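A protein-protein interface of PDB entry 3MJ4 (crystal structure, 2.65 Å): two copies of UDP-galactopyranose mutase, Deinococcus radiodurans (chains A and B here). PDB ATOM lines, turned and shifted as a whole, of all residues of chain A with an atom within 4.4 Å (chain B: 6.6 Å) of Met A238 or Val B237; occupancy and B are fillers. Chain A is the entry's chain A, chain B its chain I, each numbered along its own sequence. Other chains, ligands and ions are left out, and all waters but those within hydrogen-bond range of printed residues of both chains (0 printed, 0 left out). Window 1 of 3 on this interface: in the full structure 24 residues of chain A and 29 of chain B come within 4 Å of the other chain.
Met B238 touches Leu A56 (CE to CD1, 3.5 Å).
Lys A236 touches Met B238.
Val A237 touches Val B237.
CA of Met B238 touches O of Val A237, at 3.2 Å.
Leu B56 touches Met A238.
Met A238 touches Lys B236 (CE to CB, 3.6 Å).
Met A238 touches Val B237.
CD of Lys B236 touches OG1 of Thr A241, 3.5 Å away.
Of the printed residues of chain B, Lys A236 touches Met B238.
Met A238 touches three residues of chain B.
Of the printed residues of chain B, Leu A239 touches Val B237.
Asp B59 touches none of the printed residues of chain A.
Leu B230 touches none of the printed residues of chain A.
Val B237 touches just these residues of chain A: Val A237, Met A238 and Leu A239.
Of the printed residues of chain A, Met B238 touches Leu A56 (3.5 Å), Lys A236 (3.5 Å) and Val A237 (3.2 Å).
The nearest printed residue of chain A that does not touch Val B237 is Thr A241 (4.7 Å).
OG1 of Thr A241 is in hydrogen-bond range of O of Leu A239 (3.0 Å).
O of Ile A57 is in hydrogen-bond range of N of Met A238 (2.7 Å).
The backbone carbonyl oxygen of Val B55 lies within hydrogen-bond range of the backbone NH of Lys B236 (2.8 Å).
The backbone NH (N) of Ile B57 sits at hydrogen-bond distance from the backbone carbonyl oxygen (O) of Lys B236 (2.7 Å).
The backbone NH of Asp A59 is in hydrogen-bond range of the backbone carbonyl oxygen of Met A238, 3.0 Å away.
The backbone NH (N) of Asp B59 is in hydrogen-bond range of the backbone carbonyl oxygen (O) of Met B238 (2.9 Å).
O of Val B237 sits at hydrogen-bond distance from N of Leu A239 (2.9 Å).
The backbone NH (N) of Leu B239 is in hydrogen-bond range of the backbone carbonyl oxygen (O) of Val A237 (2.8 Å).
Of the 16 printed residues of chain B, 5 touch a printed residue of chain A.
Hydrophobic or aromatic side chains of chain B that line the printed part of chain A: Leu B56 and Met B238.
Among the printed residues, 10 pairs touch across the chains.
Among the printed residues, no Asp or Glu carboxylate lies within 4 Å of a Lys or Arg side-chain nitrogen of the other chain.
Leu A56 touches Met B238, and with the chains exchanged Met A238 touches Leu B56.
Lys A236 touches Met B238, and with the chains exchanged Met A238 touches Lys B236.
Val B237 touches its own counterpart, Val A237.
Val A237 touches Met B238, and with the chains exchanged Met A238 touches Val B237.
Positions printed for both chains: 56, 57, 58, 59, 236, 237, 238 and 239.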
ATOM      1  N   LEU A  56     -19.781 -36.746  13.020  1.00  0.00           N
ATOM      2  CA  LEU A  56     -18.755 -35.736  13.151  1.00  0.00           C
ATOM      3  C   LEU A  56     -18.731 -34.932  11.842  1.00  0.00           C
ATOM      4  O   LEU A  56     -18.604 -35.504  10.742  1.00  0.00           O
ATOM      5  CB  LEU A  56     -17.394 -36.378  13.449  1.00  0.00           C
ATOM      6  CG  LEU A  56     -16.169 -35.470  13.483  1.00  0.00           C
ATOM      7  CD1 LEU A  56     -16.252 -34.424  14.581  1.00  0.00           C
ATOM      8  CD2 LEU A  56     -14.931 -36.311  13.675  1.00  0.00           C
ATOM      9  N   ILE A  57     -18.885 -33.615  11.956  1.00  0.00           N
ATOM     10  CA  ILE A  57     -18.829 -32.736  10.785  1.00  0.00           C
ATOM     11  C   ILE A  57     -17.608 -31.827  10.919  1.00  0.00           C
ATOM     12  O   ILE A  57     -17.423 -31.173  11.958  1.00  0.00           O
ATOM     13  CB  ILE A  57     -20.167 -31.940  10.565  1.00  0.00           C
ATOM     14  CG1 ILE A  57     -20.212 -31.314   9.168  1.00  0.00           C
ATOM     15  CG2 ILE A  57     -20.411 -30.885  11.666  1.00  0.00           C
ATOM     16  CD1 ILE A  57     -21.612 -30.749   8.768  1.00  0.00           C
ATOM     17  N   VAL A  58     -16.754 -31.834   9.893  1.00  0.00           N
ATOM     18  CA  VAL A  58     -15.489 -31.125   9.943  1.00  0.00           C
ATOM     19  C   VAL A  58     -15.420 -30.134   8.805  1.00  0.00           C
ATOM     20  O   VAL A  58     -15.944 -30.382   7.719  1.00  0.00           O
ATOM     21  CB  VAL A  58     -14.304 -32.081   9.769  1.00  0.00           C
ATOM     22  CG1 VAL A  58     -14.215 -33.046  10.929  1.00  0.00           C
ATOM     23  CG2 VAL A  58     -14.461 -32.848   8.488  1.00  0.00           C
ATOM     24  N   ASP A  59     -14.754 -29.015   9.042  1.00  0.00           N
ATOM     25  CA  ASP A  59     -14.519 -28.086   7.971  1.00  0.00           C
ATOM     26  C   ASP A  59     -13.177 -27.451   8.156  1.00  0.00           C
ATOM     27  O   ASP A  59     -12.817 -27.071   9.255  1.00  0.00           O
ATOM     28  CB  ASP A  59     -15.607 -27.005   7.908  1.00  0.00           C
ATOM     29  CG  ASP A  59     -15.689 -26.359   6.549  1.00  0.00           C
ATOM     30  OD1 ASP A  59     -14.761 -25.592   6.215  1.00  0.00           O
ATOM     31  OD2 ASP A  59     -16.649 -26.654   5.805  1.00  0.00           O
ATOM     32  N   LYS A 236     -21.362 -33.625  16.243  1.00  0.00           N
ATOM     33  CA  LYS A 236     -20.194 -32.963  16.838  1.00  0.00           C
ATOM     34  C   LYS A 236     -19.600 -32.151  15.720  1.00  0.00           C
ATOM     35  O   LYS A 236     -19.466 -32.645  14.596  1.00  0.00           O
ATOM     36  CB  LYS A 236     -19.158 -33.964  17.368  1.00  0.00           C
ATOM     37  CG  LYS A 236     -19.711 -35.095  18.221  1.00  0.00           C
ATOM     38  CD  LYS A 236     -20.351 -34.578  19.477  1.00  0.00           C
ATOM     39  CE  LYS A 236     -21.862 -34.809  19.490  1.00  0.00           C
ATOM     40  NZ  LYS A 236     -22.505 -34.271  20.740  1.00  0.00           N
ATOM     41  N   VAL A 237     -19.257 -30.904  16.016  1.00  0.00           N
ATOM     42  CA  VAL A 237     -18.772 -29.995  14.992  1.00  0.00           C
ATOM     43  C   VAL A 237     -17.311 -29.652  15.214  1.00  0.00           C
ATOM     44  O   VAL A 237     -16.905 -29.267  16.318  1.00  0.00           O
ATOM     45  CB  VAL A 237     -19.573 -28.707  14.977  1.00  0.00           C
ATOM     46  CG1 VAL A 237     -19.069 -27.811  13.875  1.00  0.00           C
ATOM     47  CG2 VAL A 237     -21.043 -29.029  14.802  1.00  0.00           C
ATOM     48  N   MET A 238     -16.521 -29.787  14.155  1.00  0.00           N
ATOM     49  CA  MET A 238     -15.089 -29.645  14.282  1.00  0.00           C
ATOM     50  C   MET A 238     -14.547 -28.720  13.213  1.00  0.00           C
ATOM     51  O   MET A 238     -14.522 -29.079  12.035  1.00  0.00           O
ATOM     52  CB  MET A 238     -14.412 -31.017  14.211  1.00  0.00           C
ATOM     53  CG  MET A 238     -12.953 -31.001  14.631  1.00  0.00           C
ATOM     54  SD  MET A 238     -12.160 -32.615  14.567  1.00  0.00           S
ATOM     55  CE  MET A 238     -10.685 -32.211  15.474  1.00  0.00           C
ATOM     56  N   LEU A 239     -14.091 -27.543  13.645  1.00  0.00           N
ATOM     57  CA  LEU A 239     -13.626 -26.494  12.748  1.00  0.00           C
ATOM     58  C   LEU A 239     -12.093 -26.314  12.733  1.00  0.00           C
ATOM     59  O   LEU A 239     -11.391 -26.739  13.655  1.00  0.00           O
ATOM     60  CB  LEU A 239     -14.337 -25.190  13.100  1.00  0.00           C
ATOM     61  CG  LEU A 239     -15.856 -25.346  12.968  1.00  0.00           C
ATOM     62  CD1 LEU A 239     -16.618 -24.385  13.844  1.00  0.00           C
ATOM     63  CD2 LEU A 239     -16.286 -25.200  11.527  1.00  0.00           C
ATOM     64  N   THR A 241     -10.101 -27.645  10.499  1.00  0.00           N
ATOM     65  CA  THR A 241      -9.698 -29.032  10.438  1.00  0.00           C
ATOM     66  C   THR A 241      -9.870 -29.614   9.058  1.00  0.00           C
ATOM     67  O   THR A 241     -10.992 -29.786   8.606  1.00  0.00           O
ATOM     68  CB  THR A 241     -10.563 -29.880  11.398  1.00  0.00           C
ATOM     69  OG1 THR A 241     -10.339 -29.446  12.741  1.00  0.00           O
ATOM     70  CG2 THR A 241     -10.239 -31.369  11.279  1.00  0.00           C
ATOM     71  N   ILE A 246      -7.364 -35.641  10.610  1.00  0.00           N
ATOM     72  CA  ILE A 246      -7.918 -36.517  11.653  1.00  0.00           C
ATOM     73  C   ILE A 246      -8.298 -37.916  11.199  1.00  0.00           C
ATOM     74  O   ILE A 246      -8.584 -38.775  12.036  1.00  0.00           O
ATOM     75  CB  ILE A 246      -9.208 -35.957  12.295  1.00  0.00           C
ATOM     76  CG1 ILE A 246     -10.292 -35.828  11.225  1.00  0.00           C
ATOM     77  CG2 ILE A 246      -8.942 -34.657  13.041  1.00  0.00           C
ATOM     78  CD1 ILE A 246     -11.613 -35.484  11.776  1.00  0.00           C
ATOM     79  N   PHE B  30      -3.039 -35.991  19.162  1.00  0.00           N
ATOM     80  CA  PHE B  30      -2.783 -34.679  19.772  1.00  0.00           C
ATOM     81  C   PHE B  30      -1.881 -34.754  20.997  1.00  0.00           C
ATOM     82  O   PHE B  30      -1.823 -35.773  21.693  1.00  0.00           O
ATOM     83  CB  PHE B  30      -4.093 -34.016  20.222  1.00  0.00           C
ATOM     84  CG  PHE B  30      -5.103 -33.843  19.138  1.00  0.00           C
ATOM     85  CD1 PHE B  30      -6.146 -34.744  19.000  1.00  0.00           C
ATOM     86  CD2 PHE B  30      -5.041 -32.750  18.286  1.00  0.00           C
ATOM     87  CE1 PHE B  30      -7.102 -34.570  18.009  1.00  0.00           C
ATOM     88  CE2 PHE B  30      -5.978 -32.567  17.296  1.00  0.00           C
ATOM     89  CZ  PHE B  30      -7.018 -33.475  17.154  1.00  0.00           C
ATOM     90  N   ALA B  37     -13.592 -24.019  26.155  1.00  0.00           N
ATOM     91  CA  ALA B  37     -13.070 -22.983  25.278  1.00  0.00           C
ATOM     92  C   ALA B  37     -13.313 -21.568  25.816  1.00  0.00           C
ATOM     93  O   ALA B  37     -13.494 -20.616  25.064  1.00  0.00           O
ATOM     94  CB  ALA B  37     -13.647 -23.135  23.895  1.00  0.00           C
ATOM     95  N   VAL B  55      -3.058 -29.380  19.390  1.00  0.00           N
ATOM     96  CA  VAL B  55      -4.083 -29.113  20.378  1.00  0.00           C
ATOM     97  C   VAL B  55      -5.487 -29.369  19.863  1.00  0.00           C
ATOM     98  O   VAL B  55      -5.864 -28.910  18.798  1.00  0.00           O
ATOM     99  CB  VAL B  55      -3.965 -27.665  20.869  1.00  0.00           C
ATOM    100  CG1 VAL B  55      -5.027 -27.347  21.899  1.00  0.00           C
ATOM    101  CG2 VAL B  55      -2.571 -27.436  21.441  1.00  0.00           C
ATOM    102  N   LEU B  56      -6.263 -30.117  20.624  1.00  0.00           N
ATOM    103  CA  LEU B  56      -7.665 -30.258  20.315  1.00  0.00           C
ATOM    104  C   LEU B  56      -8.464 -29.644  21.469  1.00  0.00           C
ATOM    105  O   LEU B  56      -8.474 -30.187  22.595  1.00  0.00           O
ATOM    106  CB  LEU B  56      -8.030 -31.725  20.114  1.00  0.00           C
ATOM    107  CG  LEU B  56      -9.528 -32.026  20.079  1.00  0.00           C
ATOM    108  CD1 LEU B  56     -10.222 -31.381  18.859  1.00  0.00           C
ATOM    109  CD2 LEU B  56      -9.751 -33.536  20.131  1.00  0.00           C
ATOM    110  N   ILE B  57      -9.094 -28.495  21.202  1.00  0.00           N
ATOM    111  CA  ILE B  57      -9.911 -27.845  22.217  1.00  0.00           C
ATOM    112  C   ILE B  57     -11.386 -28.200  22.015  1.00  0.00           C
ATOM    113  O   ILE B  57     -11.868 -28.324  20.899  1.00  0.00           O
ATOM    114  CB  ILE B  57      -9.639 -26.323  22.360  1.00  0.00           C
ATOM    115  CG1 ILE B  57     -10.571 -25.726  23.419  1.00  0.00           C
ATOM    116  CG2 ILE B  57      -9.809 -25.606  21.036  1.00  0.00           C
ATOM    117  CD1 ILE B  57     -10.082 -24.462  24.042  1.00  0.00           C
ATOM    118  N   VAL B  58     -12.082 -28.388  23.123  1.00  0.00           N
ATOM    119  CA  VAL B  58     -13.376 -29.024  23.132  1.00  0.00           C
ATOM    120  C   VAL B  58     -14.352 -28.272  24.045  1.00  0.00           C
ATOM    121  O   VAL B  58     -14.012 -27.879  25.164  1.00  0.00           O
ATOM    122  CB  VAL B  58     -13.211 -30.470  23.638  1.00  0.00           C
ATOM    123  CG1 VAL B  58     -14.406 -30.896  24.457  1.00  0.00           C
ATOM    124  CG2 VAL B  58     -12.935 -31.438  22.473  1.00  0.00           C
ATOM    125  N   ASP B  59     -15.569 -28.057  23.566  1.00  0.00           N
ATOM    126  CA  ASP B  59     -16.586 -27.486  24.421  1.00  0.00           C
ATOM    127  C   ASP B  59     -17.941 -28.130  24.230  1.00  0.00           C
ATOM    128  O   ASP B  59     -18.306 -28.539  23.139  1.00  0.00           O
ATOM    129  CB  ASP B  59     -16.672 -25.977  24.280  1.00  0.00           C
ATOM    130  CG  ASP B  59     -17.165 -25.317  25.551  1.00  0.00           C
ATOM    131  OD1 ASP B  59     -18.363 -25.513  25.875  1.00  0.00           O
ATOM    132  OD2 ASP B  59     -16.358 -24.623  26.225  1.00  0.00           O
ATOM    133  N   ILE B  64     -17.325 -20.955  21.160  1.00  0.00           N
ATOM    134  CA  ILE B  64     -16.142 -20.777  21.999  1.00  0.00           C
ATOM    135  C   ILE B  64     -16.330 -19.534  22.879  1.00  0.00           C
ATOM    136  O   ILE B  64     -17.376 -18.913  22.819  1.00  0.00           O
ATOM    137  CB  ILE B  64     -14.848 -20.670  21.147  1.00  0.00           C
ATOM    138  CG1 ILE B  64     -14.691 -19.255  20.581  1.00  0.00           C
ATOM    139  CG2 ILE B  64     -14.859 -21.724  20.061  1.00  0.00           C
ATOM    140  CD1 ILE B  64     -14.586 -19.199  19.102  1.00  0.00           C
ATOM    141  N   LEU B 230      -7.715 -18.747  18.809  1.00  0.00           N
ATOM    142  CA  LEU B 230      -7.747 -20.165  18.426  1.00  0.00           C
ATOM    143  C   LEU B 230      -7.378 -20.440  16.960  1.00  0.00           C
ATOM    144  O   LEU B 230      -7.570 -21.555  16.444  1.00  0.00           O
ATOM    145  CB  LEU B 230      -9.120 -20.765  18.722  1.00  0.00           C
ATOM    146  CG  LEU B 230      -9.563 -20.576  20.160  1.00  0.00           C
ATOM    147  CD1 LEU B 230     -10.904 -21.232  20.346  1.00  0.00           C
ATOM    148  CD2 LEU B 230      -8.523 -21.152  21.069  1.00  0.00           C
ATOM    149  N   SER B 231      -6.831 -19.432  16.294  1.00  0.00           N
ATOM    150  CA  SER B 231      -6.675 -19.492  14.849  1.00  0.00           C
ATOM    151  C   SER B 231      -5.472 -20.316  14.358  1.00  0.00           C
ATOM    152  O   SER B 231      -5.458 -20.731  13.197  1.00  0.00           O
ATOM    153  CB  SER B 231      -6.606 -18.084  14.280  1.00  0.00           C
ATOM    154  OG  SER B 231      -5.443 -17.453  14.775  1.00  0.00           O
ATOM    155  N   ILE B 235      -4.346 -25.789  16.343  1.00  0.00           N
ATOM    156  CA  ILE B 235      -5.535 -25.817  17.185  1.00  0.00           C
ATOM    157  C   ILE B 235      -6.735 -26.333  16.418  1.00  0.00           C
ATOM    158  O   ILE B 235      -7.171 -25.713  15.456  1.00  0.00           O
ATOM    159  CB  ILE B 235      -5.890 -24.436  17.726  1.00  0.00           C
ATOM    160  CG1 ILE B 235      -4.703 -23.821  18.456  1.00  0.00           C
ATOM    161  CG2 ILE B 235      -7.087 -24.535  18.653  1.00  0.00           C
ATOM    162  CD1 ILE B 235      -5.010 -22.491  19.077  1.00  0.00           C
ATOM    163  N   LYS B 236      -7.250 -27.480  16.844  1.00  0.00           N
ATOM    164  CA  LYS B 236      -8.476 -28.030  16.310  1.00  0.00           C
ATOM    165  C   LYS B 236      -9.569 -27.733  17.327  1.00  0.00           C
ATOM    166  O   LYS B 236      -9.376 -27.933  18.526  1.00  0.00           O
ATOM    167  CB  LYS B 236      -8.352 -29.542  16.092  1.00  0.00           C
ATOM    168  CG  LYS B 236      -7.185 -29.954  15.247  1.00  0.00           C
ATOM    169  CD  LYS B 236      -7.103 -29.091  14.032  1.00  0.00           C
ATOM    170  CE  LYS B 236      -5.778 -29.251  13.347  1.00  0.00           C
ATOM    171  NZ  LYS B 236      -5.531 -28.120  12.423  1.00  0.00           N
ATOM    172  N   VAL B 237     -10.704 -27.236  16.851  1.00  0.00           N
ATOM    173  CA  VAL B 237     -11.759 -26.757  17.741  1.00  0.00           C
ATOM    174  C   VAL B 237     -12.959 -27.646  17.545  1.00  0.00           C
ATOM    175  O   VAL B 237     -13.422 -27.828  16.424  1.00  0.00           O
ATOM    176  CB  VAL B 237     -12.161 -25.293  17.424  1.00  0.00           C
ATOM    177  CG1 VAL B 237     -13.176 -24.785  18.440  1.00  0.00           C
ATOM    178  CG2 VAL B 237     -10.914 -24.376  17.370  1.00  0.00           C
ATOM    179  N   MET B 238     -13.442 -28.226  18.636  1.00  0.00           N
ATOM    180  CA  MET B 238     -14.594 -29.113  18.583  1.00  0.00           C
ATOM    181  C   MET B 238     -15.720 -28.598  19.502  1.00  0.00           C
ATOM    182  O   MET B 238     -15.522 -28.431  20.706  1.00  0.00           O
ATOM    183  CB  MET B 238     -14.163 -30.535  18.944  1.00  0.00           C
ATOM    184  CG  MET B 238     -15.180 -31.630  18.584  1.00  0.00           C
ATOM    185  SD  MET B 238     -14.427 -33.269  18.712  1.00  0.00           S
ATOM    186  CE  MET B 238     -15.719 -34.301  18.038  1.00  0.00           C
ATOM    187  N   LEU B 239     -16.892 -28.337  18.928  1.00  0.00           N
ATOM    188  CA  LEU B 239     -17.992 -27.728  19.673  1.00  0.00           C
ATOM    189  C   LEU B 239     -19.143 -28.705  19.731  1.00  0.00           C
ATOM    190  O   LEU B 239     -19.146 -29.674  18.986  1.00  0.00           O
ATOM    191  CB  LEU B 239     -18.453 -26.425  19.001  1.00  0.00           C
ATOM    192  CG  LEU B 239     -17.355 -25.385  18.796  1.00  0.00           C
ATOM    193  CD1 LEU B 239     -17.885 -24.130  18.105  1.00  0.00           C
ATOM    194  CD2 LEU B 239     -16.681 -25.048  20.120  1.00  0.00           C
ATOM    195  N   ILE B 250      -9.783 -40.572  20.901  1.00  0.00           N
ATOM    196  CA  ILE B 250      -8.896 -39.537  20.389  1.00  0.00           C
ATOM    197  C   ILE B 250      -7.586 -39.567  21.177  1.00  0.00           C
ATOM    198  O   ILE B 250      -7.568 -39.335  22.378  1.00  0.00           O
ATOM    199  CB  ILE B 250      -9.549 -38.137  20.471  1.00  0.00           C
ATOM    200  CG1 ILE B 250     -10.920 -38.149  19.797  1.00  0.00           C
ATOM    201  CG2 ILE B 250      -8.643 -37.084  19.828  1.00  0.00           C
ATOM    202  CD1 ILE B 250     -10.866 -37.793  18.343  1.00  0.00           C
